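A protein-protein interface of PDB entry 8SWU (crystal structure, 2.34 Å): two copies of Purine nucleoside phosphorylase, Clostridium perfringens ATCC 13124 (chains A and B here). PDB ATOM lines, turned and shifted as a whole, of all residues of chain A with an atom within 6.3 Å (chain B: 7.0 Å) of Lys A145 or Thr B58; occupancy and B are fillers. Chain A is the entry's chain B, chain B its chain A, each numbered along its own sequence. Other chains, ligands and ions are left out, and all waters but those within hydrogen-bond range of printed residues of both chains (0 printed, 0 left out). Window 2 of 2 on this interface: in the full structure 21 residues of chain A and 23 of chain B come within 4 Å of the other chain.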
ATOM      1  N   LEU A 142     -27.784   6.072 -28.273  1.00  0.00           N
ATOM      2  CA  LEU A 142     -26.826   5.277 -27.515  1.00  0.00           C
ATOM      3  C   LEU A 142     -25.377   5.604 -27.846  1.00  0.00           C
ATOM      4  O   LEU A 142     -24.475   4.998 -27.260  1.00  0.00           O
ATOM      5  CB  LEU A 142     -27.077   3.785 -27.745  1.00  0.00           C
ATOM      6  CG  LEU A 142     -28.264   3.193 -26.986  1.00  0.00           C
ATOM      7  CD1 LEU A 142     -28.553   1.781 -27.469  1.00  0.00           C
ATOM      8  CD2 LEU A 142     -27.995   3.213 -25.493  1.00  0.00           C
ATOM      9  N   ILE A 143     -25.129   6.536 -28.771  1.00  0.00           N
ATOM     10  CA  ILE A 143     -23.758   6.909 -29.096  1.00  0.00           C
ATOM     11  C   ILE A 143     -23.114   7.556 -27.880  1.00  0.00           C
ATOM     12  O   ILE A 143     -23.692   8.451 -27.250  1.00  0.00           O
ATOM     13  CB  ILE A 143     -23.732   7.837 -30.320  1.00  0.00           C
ATOM     14  CG1 ILE A 143     -23.864   7.023 -31.610  1.00  0.00           C
ATOM     15  CG2 ILE A 143     -22.453   8.664 -30.343  1.00  0.00           C
ATOM     16  CD1 ILE A 143     -24.226   7.854 -32.825  1.00  0.00           C
ATOM     17  N   GLY A 144     -21.923   7.095 -27.534  1.00  0.00           N
ATOM     18  CA  GLY A 144     -21.226   7.534 -26.344  1.00  0.00           C
ATOM     19  C   GLY A 144     -20.885   6.359 -25.453  1.00  0.00           C
ATOM     20  O   GLY A 144     -21.036   5.192 -25.828  1.00  0.00           O
ATOM     21  N   LYS A 145     -20.413   6.678 -24.253  1.00  0.00           N
ATOM     22  CA  LYS A 145     -20.054   5.638 -23.299  1.00  0.00           C
ATOM     23  C   LYS A 145     -21.294   4.858 -22.885  1.00  0.00           C
ATOM     24  O   LYS A 145     -22.330   5.445 -22.556  1.00  0.00           O
ATOM     25  CB  LYS A 145     -19.374   6.250 -22.076  1.00  0.00           C
ATOM     26  CG  LYS A 145     -18.217   5.422 -21.543  1.00  0.00           C
ATOM     27  CD  LYS A 145     -17.999   5.667 -20.062  1.00  0.00           C
ATOM     28  CE  LYS A 145     -17.354   4.463 -19.397  1.00  0.00           C
ATOM     29  NZ  LYS A 145     -18.371   3.472 -18.949  1.00  0.00           N
ATOM     30  N   ASN A 146     -21.191   3.533 -22.909  1.00  0.00           N
ATOM     31  CA  ASN A 146     -22.326   2.694 -22.557  1.00  0.00           C
ATOM     32  C   ASN A 146     -22.600   2.752 -21.059  1.00  0.00           C
ATOM     33  O   ASN A 146     -21.679   2.716 -20.238  1.00  0.00           O
ATOM     34  CB  ASN A 146     -22.075   1.249 -22.985  1.00  0.00           C
ATOM     35  CG  ASN A 146     -23.303   0.373 -22.823  1.00  0.00           C
ATOM     36  OD1 ASN A 146     -24.361   0.655 -23.386  1.00  0.00           O
ATOM     37  ND2 ASN A 146     -23.171  -0.694 -22.045  1.00  0.00           N
ATOM     38  N   LEU A 147     -23.882   2.845 -20.707  1.00  0.00           N
ATOM     39  CA  LEU A 147     -24.319   2.766 -19.315  1.00  0.00           C
ATOM     40  C   LEU A 147     -24.506   1.294 -18.977  1.00  0.00           C
ATOM     41  O   LEU A 147     -25.539   0.700 -19.292  1.00  0.00           O
ATOM     42  CB  LEU A 147     -25.610   3.549 -19.101  1.00  0.00           C
ATOM     43  CG  LEU A 147     -25.705   4.951 -19.701  1.00  0.00           C
ATOM     44  CD1 LEU A 147     -27.037   5.588 -19.331  1.00  0.00           C
ATOM     45  CD2 LEU A 147     -24.536   5.814 -19.244  1.00  0.00           C
ATOM     46  N   ASN A 148     -23.502   0.700 -18.327  1.00  0.00           N
ATOM     47  CA  ASN A 148     -23.545  -0.733 -18.052  1.00  0.00           C
ATOM     48  C   ASN A 148     -24.661  -1.094 -17.081  1.00  0.00           C
ATOM     49  O   ASN A 148     -25.156  -2.228 -17.105  1.00  0.00           O
ATOM     50  CB  ASN A 148     -22.195  -1.199 -17.507  1.00  0.00           C
ATOM     51  CG  ASN A 148     -21.072  -1.006 -18.502  1.00  0.00           C
ATOM     52  OD1 ASN A 148     -21.310  -0.697 -19.670  1.00  0.00           O
ATOM     53  ND2 ASN A 148     -19.838  -1.187 -18.047  1.00  0.00           N
ATOM     54  N   ARG A 153     -23.393  -3.147 -24.493  1.00  0.00           N
ATOM     55  CA  ARG A 153     -22.846  -2.157 -25.417  1.00  0.00           C
ATOM     56  C   ARG A 153     -23.501  -2.254 -26.791  1.00  0.00           C
ATOM     57  O   ARG A 153     -23.760  -1.230 -27.434  1.00  0.00           O
ATOM     58  CB  ARG A 153     -21.329  -2.324 -25.525  1.00  0.00           C
ATOM     59  CG  ARG A 153     -20.701  -1.650 -26.743  1.00  0.00           C
ATOM     60  CD  ARG A 153     -20.330  -0.200 -26.454  1.00  0.00           C
ATOM     61  NE  ARG A 153     -21.473   0.696 -26.583  1.00  0.00           N
ATOM     62  CZ  ARG A 153     -21.417   2.013 -26.430  1.00  0.00           C
ATOM     63  NH1 ARG A 153     -20.282   2.628 -26.145  1.00  0.00           N
ATOM     64  NH2 ARG A 153     -22.528   2.730 -26.565  1.00  0.00           N
ATOM     65  N   VAL B  56      -8.498   9.184 -25.608  1.00  0.00           N
ATOM     66  CA  VAL B  56      -8.560   8.389 -24.388  1.00  0.00           C
ATOM     67  C   VAL B  56      -9.641   7.327 -24.536  1.00  0.00           C
ATOM     68  O   VAL B  56     -10.729   7.593 -25.062  1.00  0.00           O
ATOM     69  CB  VAL B  56      -8.827   9.294 -23.170  1.00  0.00           C
ATOM     70  CG1 VAL B  56      -8.571   8.536 -21.875  1.00  0.00           C
ATOM     71  CG2 VAL B  56      -7.974  10.552 -23.244  1.00  0.00           C
ATOM     72  N   SER B  57      -9.344   6.117 -24.075  1.00  0.00           N
ATOM     73  CA  SER B  57     -10.281   5.005 -24.131  1.00  0.00           C
ATOM     74  C   SER B  57     -11.161   4.981 -22.883  1.00  0.00           C
ATOM     75  O   SER B  57     -10.847   5.584 -21.853  1.00  0.00           O
ATOM     76  CB  SER B  57      -9.539   3.679 -24.289  1.00  0.00           C
ATOM     77  OG  SER B  57      -9.000   3.544 -25.596  1.00  0.00           O
ATOM     78  N   THR B  58     -12.284   4.277 -22.995  1.00  0.00           N
ATOM     79  CA  THR B  58     -13.233   4.116 -21.892  1.00  0.00           C
ATOM     80  C   THR B  58     -13.119   2.715 -21.293  1.00  0.00           C
ATOM     81  O   THR B  58     -14.083   1.948 -21.237  1.00  0.00           O
ATOM     82  CB  THR B  58     -14.655   4.398 -22.372  1.00  0.00           C
ATOM     83  OG1 THR B  58     -14.986   3.499 -23.434  1.00  0.00           O
ATOM     84  CG2 THR B  58     -14.773   5.828 -22.866  1.00  0.00           C
ATOM     85  N   PHE B  83     -10.651   2.890 -32.898  1.00  0.00           N
ATOM     86  CA  PHE B  83     -11.636   3.746 -32.253  1.00  0.00           C
ATOM     87  C   PHE B  83     -12.889   3.824 -33.113  1.00  0.00           C
ATOM     88  O   PHE B  83     -12.809   3.946 -34.339  1.00  0.00           O
ATOM     89  CB  PHE B  83     -11.068   5.146 -32.015  1.00  0.00           C
ATOM     90  CG  PHE B  83      -9.839   5.160 -31.152  1.00  0.00           C
ATOM     91  CD1 PHE B  83      -9.945   5.214 -29.773  1.00  0.00           C
ATOM     92  CD2 PHE B  83      -8.576   5.110 -31.721  1.00  0.00           C
ATOM     93  CE1 PHE B  83      -8.816   5.221 -28.975  1.00  0.00           C
ATOM     94  CE2 PHE B  83      -7.443   5.117 -30.930  1.00  0.00           C
ATOM     95  CZ  PHE B  83      -7.564   5.174 -29.555  1.00  0.00           C
ATOM     96  N   TYR B  86     -19.311   5.084 -32.521  1.00  0.00           N
ATOM     97  CA  TYR B  86     -20.397   4.843 -31.579  1.00  0.00           C
ATOM     98  C   TYR B  86     -19.991   5.042 -30.124  1.00  0.00           C
ATOM     99  O   TYR B  86     -20.873   5.120 -29.264  1.00  0.00           O
ATOM    100  CB  TYR B  86     -20.979   3.431 -31.761  1.00  0.00           C
ATOM    101  CG  TYR B  86     -20.004   2.272 -31.618  1.00  0.00           C
ATOM    102  CD1 TYR B  86     -19.408   1.971 -30.396  1.00  0.00           C
ATOM    103  CD2 TYR B  86     -19.710   1.457 -32.704  1.00  0.00           C
ATOM    104  CE1 TYR B  86     -18.526   0.908 -30.269  1.00  0.00           C
ATOM    105  CE2 TYR B  86     -18.840   0.391 -32.587  1.00  0.00           C
ATOM    106  CZ  TYR B  86     -18.247   0.121 -31.370  1.00  0.00           C
ATOM    107  OH  TYR B  86     -17.374  -0.939 -31.259  1.00  0.00           O
ATOM    108  N   GLU B  87     -18.692   5.117 -29.825  1.00  0.00           N
ATOM    109  CA  GLU B  87     -18.248   5.310 -28.449  1.00  0.00           C
ATOM    110  C   GLU B  87     -18.260   6.769 -28.015  1.00  0.00           C
ATOM    111  O   GLU B  87     -18.013   7.047 -26.836  1.00  0.00           O
ATOM    112  CB  GLU B  87     -16.842   4.733 -28.251  1.00  0.00           C
ATOM    113  CG  GLU B  87     -16.804   3.215 -28.127  1.00  0.00           C
ATOM    114  CD  GLU B  87     -17.193   2.729 -26.738  1.00  0.00           C
ATOM    115  OE1 GLU B  87     -16.973   3.473 -25.757  1.00  0.00           O
ATOM    116  OE2 GLU B  87     -17.725   1.603 -26.627  1.00  0.00           O
ATOM    117  N   GLY B  88     -18.536   7.699 -28.923  1.00  0.00           N
ATOM    118  CA  GLY B  88     -18.593   9.113 -28.596  1.00  0.00           C
ATOM    119  C   GLY B  88     -17.517   9.967 -29.236  1.00  0.00           C
ATOM    120  O   GLY B  88     -17.647  11.201 -29.227  1.00  0.00           O
ATOM    121  N   TYR B  89     -16.460   9.379 -29.790  1.00  0.00           N
ATOM    122  CA  TYR B  89     -15.425  10.166 -30.445  1.00  0.00           C
ATOM    123  C   TYR B  89     -15.980  10.879 -31.673  1.00  0.00           C
ATOM    124  O   TYR B  89     -16.852  10.364 -32.378  1.00  0.00           O
ATOM    125  CB  TYR B  89     -14.255   9.277 -30.871  1.00  0.00           C
ATOM    126  CG  TYR B  89     -13.671   8.426 -29.770  1.00  0.00           C
ATOM    127  CD1 TYR B  89     -12.840   8.979 -28.804  1.00  0.00           C
ATOM    128  CD2 TYR B  89     -13.938   7.064 -29.707  1.00  0.00           C
ATOM    129  CE1 TYR B  89     -12.302   8.199 -27.797  1.00  0.00           C
ATOM    130  CE2 TYR B  89     -13.402   6.276 -28.704  1.00  0.00           C
ATOM    131  CZ  TYR B  89     -12.586   6.849 -27.752  1.00  0.00           C
ATOM    132  OH  TYR B  89     -12.054   6.069 -26.754  1.00  0.00           O
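OE2 of Glu B87 lies within salt-bridge range of NH1 of Arg A153 (2.8 Å). N of Gly A144 is in hydrogen-bond range of O of Tyr B86 (2.8 Å).
Of the printed residues of chain A, Thr B58 touches Lys A145. Of the printed residues of chain A, Gly B88 touches Gly A144 (3.7 Å). Of the printed residues of chain B, Ile A143 touches Tyr B86 (3.4 Å). Val B56 touches none of the printed residues of chain A. Leu A142 touches none of the printed residues of chain B. The nearest residue of chain A that does not touch Thr B58 is Arg A153 (6.0 Å). The nearest printed residue of chain B that does not touch Arg A153 is Thr B58 (6.0 Å).
No position is printed for both chains.
Tyr B86 touches Ile A143 (O to CA, 3.4 Å). Glu B87 touches Gly A144. N of Gly A144 touches N of Gly B88, 3.7 Å away. Lys A145 touches Thr B58 (CG to CG2, 3.7 Å). Lys A145 touches Glu B87. NH2 of Arg A153 touches O of Tyr B86, 3.97 Å away.
Of the 8 printed residues of chain A, 4 touch a printed residue of chain B. Printed residues of chain A that touch a printed residue of chain B: Ile A143, Gly A144, Lys A145 and Arg A153. Printed residues of chain B that touch a printed residue of chain A: Thr B58, Tyr B86, Glu B87 and Gly B88. Along chain B the printed residues that touch a printed residue of chain A span positions 58 to 88. Among the printed residues, 8 pairs touch across the chains. Among the printed residues, Asp or Glu carboxylates within 4 Å of a Lys or Arg side-chain nitrogen of the other chain: Arg A153 with Glu B87.
O of Gly A144 is in hydrogen-bond range of NH1 of Arg A153. The side-chain carboxylate of Glu B87 lies within hydrogen-bond range of the side-chain hydroxyl of Thr B58, 3.1 Å away. The side-chain amide nitrogen (ND2) of Asn A146 lies close to the backbone NH (N) of Arg A153 (3.5 Å). The backbone carbonyl oxygen (O) of Leu A142 sits at hydrogen-bond distance from the guanidinium group (NH2) of Arg A153 (3.1 Å).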
